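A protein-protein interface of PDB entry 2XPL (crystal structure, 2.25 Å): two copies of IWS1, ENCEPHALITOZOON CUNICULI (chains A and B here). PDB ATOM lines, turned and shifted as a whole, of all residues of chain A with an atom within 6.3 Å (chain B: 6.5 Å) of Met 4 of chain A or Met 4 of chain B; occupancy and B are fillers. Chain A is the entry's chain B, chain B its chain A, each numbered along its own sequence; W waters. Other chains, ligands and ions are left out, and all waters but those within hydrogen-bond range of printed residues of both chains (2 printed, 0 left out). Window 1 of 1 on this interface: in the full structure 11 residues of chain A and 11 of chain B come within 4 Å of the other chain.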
ATOM      1  N   HIS A   3       7.127   1.822 -17.407  1.00  0.00           N
ATOM      2  CA  HIS A   3       5.892   1.726 -16.555  1.00  0.00           C
ATOM      3  C   HIS A   3       5.571   2.983 -15.707  1.00  0.00           C
ATOM      4  O   HIS A   3       4.708   3.755 -16.084  1.00  0.00           O
ATOM      5  CB  HIS A   3       5.896   0.473 -15.680  1.00  0.00           C
ATOM      6  CG  HIS A   3       4.524  -0.070 -15.405  1.00  0.00           C
ATOM      7  ND1 HIS A   3       3.696  -0.551 -16.408  1.00  0.00           N
ATOM      8  CD2 HIS A   3       3.845  -0.229 -14.246  1.00  0.00           C
ATOM      9  CE1 HIS A   3       2.564  -0.976 -15.873  1.00  0.00           C
ATOM     10  NE2 HIS A   3       2.621  -0.772 -14.564  1.00  0.00           N
ATOM     11  N   MET A   4       6.233   3.196 -14.574  1.00  0.00           N
ATOM     12  CA  MET A   4       6.085   4.496 -13.866  1.00  0.00           C
ATOM     13  C   MET A   4       7.302   5.410 -14.097  1.00  0.00           C
ATOM     14  O   MET A   4       8.428   4.983 -13.867  1.00  0.00           O
ATOM     15  CB  MET A   4       5.799   4.326 -12.378  1.00  0.00           C
ATOM     16  CG  MET A   4       5.433   5.663 -11.721  1.00  0.00           C
ATOM     17  SD  MET A   4       4.957   5.665  -9.980  1.00  0.00           S
ATOM     18  CE  MET A   4       3.213   5.261 -10.112  1.00  0.00           C
ATOM     19  N   ASP A   5       7.084   6.646 -14.546  1.00  0.00           N
ATOM     20  CA  ASP A   5       8.207   7.581 -14.781  1.00  0.00           C
ATOM     21  C   ASP A   5       9.020   7.888 -13.532  1.00  0.00           C
ATOM     22  O   ASP A   5       8.489   7.900 -12.474  1.00  0.00           O
ATOM     23  CB  ASP A   5       7.687   8.869 -15.376  1.00  0.00           C
ATOM     24  CG  ASP A   5       7.199   8.677 -16.762  1.00  0.00           C
ATOM     25  OD1 ASP A   5       7.757   7.800 -17.476  1.00  0.00           O
ATOM     26  OD2 ASP A   5       6.263   9.403 -17.172  1.00  0.00           O
ATOM     27  N   PRO A   6      10.333   8.134 -13.653  1.00  0.00           N
ATOM     28  CA  PRO A   6      11.088   8.346 -12.410  1.00  0.00           C
ATOM     29  C   PRO A   6      10.675   9.626 -11.638  1.00  0.00           C
ATOM     30  O   PRO A   6      10.739   9.639 -10.412  1.00  0.00           O
ATOM     31  CB  PRO A   6      12.545   8.383 -12.878  1.00  0.00           C
ATOM     32  CG  PRO A   6      12.463   8.784 -14.320  1.00  0.00           C
ATOM     33  CD  PRO A   6      11.099   8.512 -14.857  1.00  0.00           C
ATOM     34  N   GLY A   7      10.194  10.648 -12.343  1.00  0.00           N
ATOM     35  CA  GLY A   7       9.574  11.825 -11.745  1.00  0.00           C
ATOM     36  C   GLY A   7       8.424  11.469 -10.823  1.00  0.00           C
ATOM     37  O   GLY A   7       8.321  11.993  -9.714  1.00  0.00           O
ATOM     38  N   THR A   8       7.562  10.551 -11.256  1.00  0.00           N
ATOM     39  CA  THR A   8       6.376  10.162 -10.494  1.00  0.00           C
ATOM     40  C   THR A   8       6.731   9.326  -9.271  1.00  0.00           C
ATOM     41  O   THR A   8       6.291   9.617  -8.162  1.00  0.00           O
ATOM     42  CB  THR A   8       5.383   9.424 -11.405  1.00  0.00           C
ATOM     43  OG1 THR A   8       5.197  10.194 -12.587  1.00  0.00           O
ATOM     44  CG2 THR A   8       4.031   9.300 -10.718  1.00  0.00           C
ATOM     45  N   VAL A   9       7.577   8.305  -9.464  1.00  0.00           N
ATOM     46  CA  VAL A   9       8.131   7.592  -8.332  1.00  0.00           C
ATOM     47  C   VAL A   9       8.688   8.587  -7.297  1.00  0.00           C
ATOM     48  O   VAL A   9       8.444   8.439  -6.111  1.00  0.00           O
ATOM     49  CB  VAL A   9       9.290   6.634  -8.744  1.00  0.00           C
ATOM     50  CG1 VAL A   9      10.006   6.077  -7.529  1.00  0.00           C
ATOM     51  CG2 VAL A   9       8.808   5.505  -9.627  1.00  0.00           C
ATOM     52  N   ILE A  12       5.701  10.634  -5.512  1.00  0.00           N
ATOM     53  CA  ILE A  12       4.955   9.781  -4.584  1.00  0.00           C
ATOM     54  C   ILE A  12       5.775   9.503  -3.327  1.00  0.00           C
ATOM     55  O   ILE A  12       5.252   9.563  -2.202  1.00  0.00           O
ATOM     56  CB  ILE A  12       4.578   8.472  -5.295  1.00  0.00           C
ATOM     57  CG1 ILE A  12       3.572   8.832  -6.402  1.00  0.00           C
ATOM     58  CG2 ILE A  12       4.033   7.484  -4.318  1.00  0.00           C
ATOM     59  CD1 ILE A  12       3.059   7.705  -7.225  1.00  0.00           C
ATOM     60  N   SER A  53       6.176  -1.253  -1.113  1.00  0.00           N
ATOM     61  CA  SER A  53       6.248  -1.302  -2.572  1.00  0.00           C
ATOM     62  C   SER A  53       7.685  -1.424  -3.090  1.00  0.00           C
ATOM     63  O   SER A  53       8.490  -0.525  -2.889  1.00  0.00           O
ATOM     64  CB  SER A  53       5.667  -0.035  -3.208  1.00  0.00           C
ATOM     65  OG  SER A  53       5.799  -0.165  -4.616  1.00  0.00           O
ATOM     66  N   ALA A  55       8.785  -1.020  -6.119  1.00  0.00           N
ATOM     67  CA  ALA A  55       9.074   0.046  -7.066  1.00  0.00           C
ATOM     68  C   ALA A  55       9.506   1.350  -6.377  1.00  0.00           C
ATOM     69  O   ALA A  55      10.183   2.179  -6.989  1.00  0.00           O
ATOM     70  CB  ALA A  55       7.879   0.294  -7.939  1.00  0.00           C
ATOM     71  N   LEU A  56       9.108   1.522  -5.109  1.00  0.00           N
ATOM     72  CA  LEU A  56       9.271   2.783  -4.425  1.00  0.00           C
ATOM     73  C   LEU A  56      10.405   2.745  -3.401  1.00  0.00           C
ATOM     74  O   LEU A  56      11.003   3.777  -3.095  1.00  0.00           O
ATOM     75  CB  LEU A  56       7.937   3.213  -3.755  1.00  0.00           C
ATOM     76  CG  LEU A  56       6.663   3.482  -4.603  1.00  0.00           C
ATOM     77  CD1 LEU A  56       5.495   4.025  -3.737  1.00  0.00           C
ATOM     78  CD2 LEU A  56       6.905   4.441  -5.801  1.00  0.00           C
ATOM     79  N   HIS B   3       6.974  -3.404 -13.394  1.00  0.00           N
ATOM     80  CA  HIS B   3       7.897  -3.002 -12.283  1.00  0.00           C
ATOM     81  C   HIS B   3       7.237  -2.293 -11.031  1.00  0.00           C
ATOM     82  O   HIS B   3       7.810  -2.355  -9.945  1.00  0.00           O
ATOM     83  CB  HIS B   3       9.122  -2.244 -12.829  1.00  0.00           C
ATOM     84  CG  HIS B   3       8.954  -0.759 -12.847  1.00  0.00           C
ATOM     85  ND1 HIS B   3       9.826   0.097 -12.212  1.00  0.00           N
ATOM     86  CD2 HIS B   3       8.013   0.022 -13.421  1.00  0.00           C
ATOM     87  CE1 HIS B   3       9.419   1.343 -12.375  1.00  0.00           C
ATOM     88  NE2 HIS B   3       8.323   1.325 -13.113  1.00  0.00           N
ATOM     89  N   MET B   4       6.065  -1.654 -11.182  1.00  0.00           N
ATOM     90  CA  MET B   4       5.133  -1.390 -10.024  1.00  0.00           C
ATOM     91  C   MET B   4       3.999  -2.438 -10.031  1.00  0.00           C
ATOM     92  O   MET B   4       3.337  -2.596 -11.058  1.00  0.00           O
ATOM     93  CB  MET B   4       4.552   0.045 -10.016  1.00  0.00           C
ATOM     94  CG  MET B   4       3.371   0.256  -8.995  1.00  0.00           C
ATOM     95  SD  MET B   4       2.993   1.881  -8.245  1.00  0.00           S
ATOM     96  CE  MET B   4       4.494   2.094  -7.275  1.00  0.00           C
ATOM     97  N   ASP B   5       3.803  -3.166  -8.929  1.00  0.00           N
ATOM     98  CA  ASP B   5       2.773  -4.228  -8.843  1.00  0.00           C
ATOM     99  C   ASP B   5       1.332  -3.729  -9.042  1.00  0.00           C
ATOM    100  O   ASP B   5       0.998  -2.665  -8.607  1.00  0.00           O
ATOM    101  CB  ASP B   5       2.836  -4.905  -7.480  1.00  0.00           C
ATOM    102  CG  ASP B   5       3.967  -5.866  -7.363  1.00  0.00           C
ATOM    103  OD1 ASP B   5       4.493  -6.345  -8.402  1.00  0.00           O
ATOM    104  OD2 ASP B   5       4.332  -6.193  -6.211  1.00  0.00           O
ATOM    105  N   PRO B   6       0.460  -4.524  -9.672  1.00  0.00           N
ATOM    106  CA  PRO B   6      -0.903  -4.054  -9.869  1.00  0.00           C
ATOM    107  C   PRO B   6      -1.648  -3.739  -8.567  1.00  0.00           C
ATOM    108  O   PRO B   6      -2.427  -2.799  -8.544  1.00  0.00           O
ATOM    109  CB  PRO B   6      -1.573  -5.190 -10.649  1.00  0.00           C
ATOM    110  CG  PRO B   6      -0.744  -6.351 -10.447  1.00  0.00           C
ATOM    111  CD  PRO B   6       0.639  -5.924 -10.092  1.00  0.00           C
ATOM    112  N   GLY B   7      -1.362  -4.459  -7.487  1.00  0.00           N
ATOM    113  CA  GLY B   7      -1.905  -4.137  -6.160  1.00  0.00           C
ATOM    114  C   GLY B   7      -1.448  -2.799  -5.616  1.00  0.00           C
ATOM    115  O   GLY B   7      -2.199  -2.089  -4.929  1.00  0.00           O
ATOM    116  N   THR B   8      -0.224  -2.414  -5.938  1.00  0.00           N
ATOM    117  CA  THR B   8       0.301  -1.104  -5.512  1.00  0.00           C
ATOM    118  C   THR B   8      -0.327   0.061  -6.305  1.00  0.00           C
ATOM    119  O   THR B   8      -0.804   1.069  -5.716  1.00  0.00           O
ATOM    120  CB  THR B   8       1.858  -1.116  -5.542  1.00  0.00           C
ATOM    121  OG1 THR B   8       2.309  -2.278  -4.822  1.00  0.00           O
ATOM    122  CG2 THR B   8       2.440   0.102  -4.880  1.00  0.00           C
ATOM    123  N   VAL B   9      -0.376  -0.091  -7.641  1.00  0.00           N
ATOM    124  CA  VAL B   9      -1.035   0.901  -8.460  1.00  0.00           C
ATOM    125  C   VAL B   9      -2.457   1.087  -7.912  1.00  0.00           C
ATOM    126  O   VAL B   9      -2.936   2.211  -7.818  1.00  0.00           O
ATOM    127  CB  VAL B   9      -1.136   0.484  -9.954  1.00  0.00           C
ATOM    128  CG1 VAL B   9      -2.007   1.444 -10.713  1.00  0.00           C
ATOM    129  CG2 VAL B   9       0.233   0.354 -10.604  1.00  0.00           C
ATOM    130  N   LEU B  10      -3.151  -0.009  -7.596  1.00  0.00           N
ATOM    131  CA  LEU B  10      -4.545   0.130  -7.141  1.00  0.00           C
ATOM    132  C   LEU B  10      -4.582   0.858  -5.805  1.00  0.00           C
ATOM    133  O   LEU B  10      -5.387   1.789  -5.650  1.00  0.00           O
ATOM    134  CB  LEU B  10      -5.297  -1.203  -7.061  1.00  0.00           C
ATOM    135  CG  LEU B  10      -6.758  -1.216  -6.618  1.00  0.00           C
ATOM    136  CD1 LEU B  10      -7.624  -0.244  -7.426  1.00  0.00           C
ATOM    137  CD2 LEU B  10      -7.262  -2.648  -6.799  1.00  0.00           C
ATOM    138  N   ILE B  12      -2.519   3.030  -4.351  1.00  0.00           N
ATOM    139  CA  ILE B  12      -2.179   4.413  -4.516  1.00  0.00           C
ATOM    140  C   ILE B  12      -3.317   5.171  -5.193  1.00  0.00           C
ATOM    141  O   ILE B  12      -3.632   6.314  -4.794  1.00  0.00           O
ATOM    142  CB  ILE B  12      -0.911   4.550  -5.365  1.00  0.00           C
ATOM    143  CG1 ILE B  12       0.293   4.109  -4.534  1.00  0.00           C
ATOM    144  CG2 ILE B  12      -0.745   5.954  -5.870  1.00  0.00           C
ATOM    145  CD1 ILE B  12       1.528   3.942  -5.324  1.00  0.00           C
ATOM    146  N   SER B  53      -0.072  11.040 -13.807  1.00  0.00           N
ATOM    147  CA  SER B  53       0.802   9.861 -13.999  1.00  0.00           C
ATOM    148  C   SER B  53       0.233   8.879 -15.016  1.00  0.00           C
ATOM    149  O   SER B  53      -0.839   8.298 -14.827  1.00  0.00           O
ATOM    150  CB  SER B  53       1.058   9.067 -12.720  1.00  0.00           C
ATOM    151  OG  SER B  53       1.919   7.976 -13.083  1.00  0.00           O
ATOM    152  N   ALA B  55       1.154   5.828 -15.754  1.00  0.00           N
ATOM    153  CA  ALA B  55       0.983   4.541 -15.072  1.00  0.00           C
ATOM    154  C   ALA B  55      -0.287   4.383 -14.172  1.00  0.00           C
ATOM    155  O   ALA B  55      -0.685   3.254 -13.864  1.00  0.00           O
ATOM    156  CB  ALA B  55       2.211   4.261 -14.252  1.00  0.00           C
ATOM    157  N   LEU B  56      -0.885   5.499 -13.732  1.00  0.00           N
ATOM    158  CA  LEU B  56      -1.947   5.453 -12.734  1.00  0.00           C
ATOM    159  C   LEU B  56      -3.286   5.788 -13.348  1.00  0.00           C
ATOM    160  O   LEU B  56      -4.302   5.401 -12.822  1.00  0.00           O
ATOM    161  CB  LEU B  56      -1.672   6.419 -11.550  1.00  0.00           C
ATOM    162  CG  LEU B  56      -0.459   6.213 -10.612  1.00  0.00           C
ATOM    163  CD1 LEU B  56      -0.487   7.183  -9.406  1.00  0.00           C
ATOM    164  CD2 LEU B  56      -0.312   4.779 -10.113  1.00  0.00           C
HETATM  165  O   HOH W   1       4.297   7.716 -14.440  1.00  0.00           O
HETATM  166  O   HOH W   2       5.252  -2.384  -6.572  1.00  0.00           O
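A ring nitrogen (NE2) of His 3 of chain B is in hydrogen-bond range of the backbone NH (N) of Met 4 of chain A, 3.2 Å away.
Of the 11 printed residues of chain A, 6 touch a printed residue of chain B.
Hydrophobic or aromatic side chains of chain A within 4 Å of the printed part of chain B: His 3, Met 4, Ala 55 and Leu 56.
Of the 12 printed residues of chain B, 6 touch a printed residue of chain A.
Printed residues of chain B that touch a printed residue of chain A: His 3, Met 4, Thr 8, Ser 53, Ala 55 and Leu 56.
Hydrophobic or aromatic side chains of chain B within 4 Å of the printed part of chain A: His 3, Met 4, Ala 55 and Leu 56.
Among the printed residues, no Asp or Glu carboxylate lies within 4 Å of a Lys or Arg side-chain nitrogen of the other chain.
Among the printed residues, pairs that only touch across the chains: His 3 of chain A with His 3 of chain B, His 3 of chain A with Ala 55 of chain B, Met 4 of chain A with Met 4 of chain B, Met 4 of chain A with Ala 55 of chain B, Met 4 of chain A with Leu 56 of chain B, Thr 8 of chain A with Ser 53 of chain B, Ser 53 of chain A with Met 4 of chain B, Ser 53 of chain A with Thr 8 of chain B, Ala 55 of chain A with His 3 of chain B, Ala 55 of chain A with Met 4 of chain B and Leu 56 of chain A with Met 4 of chain B.
His 3 of chain A touches its own counterpart, His 3 of chain B.
His 3 of chain A touches Ala 55 of chain B, and with the chains exchanged Ala 55 of chain A touches His 3 of chain B.
Met 4 of chain A touches Leu 56 of chain B, and with the chains exchanged Leu 56 of chain A touches Met 4 of chain B.
Ser 53 of chain A touches Met 4 of chain B, but with the chains exchanged Met 4 of chain A does not touch Ser 53 of chain B (4.2 Å).
Water W1 lies within hydrogen-bond range of the side-chain hydroxyl (OG) of Ser 53 of chain B (2.8 Å), the backbone NH (N) of Asp 5 of chain A (3.0 Å) and the side-chain hydroxyl (OG1) of Thr 8 of chain A (3.2 Å).
Water W2 lies within hydrogen-bond range of N of Asp 5 of chain B (2.9 Å), OG of Ser 53 of chain A (3.0 Å) and OG1 of Thr 8 of chain B (3.4 Å).
SD of Met 4 of chain A lies within hydrogen-bond range of N of Val 9 of chain A.
The backbone NH (N) of Ala 55 of chain A sits close to the side-chain hydroxyl (OG) of Ser 53 of chain A, 3.5 Å away.
Of chain B, only His 3 (3.2 Å), Met 4 (3.9 Å), Ala 55 (3.9 Å) and Leu 56 (3.6 Å) come within 4 Å of Met 4 of chain A.
Val 9 of chain A touches none of the printed residues of chain B.
Of the printed residues of chain B, Ser 53 of chain A touches Met 4 and Thr 8.
Printed residues of chain A within 4 Å of Met 4 of chain B: Met 4 (3.9 Å), Ser 53 (3.7 Å), Ala 55 (3.8 Å) and Leu 56 (3.7 Å).
Of the printed residues of chain A, Thr 8 of chain B touches Ser 53.
Leu 10 of chain B touches none of the printed residues of chain A.
Printed residues of chain A within 4 Å of Ala 55 of chain B: His 3 and Met 4.
Of the printed residues of chain A, Leu 56 of chain B touches Met 4.
The nearest printed residue of chain A that does not touch Met 4 of chain B is His 3 of chain A (4.003 Å).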
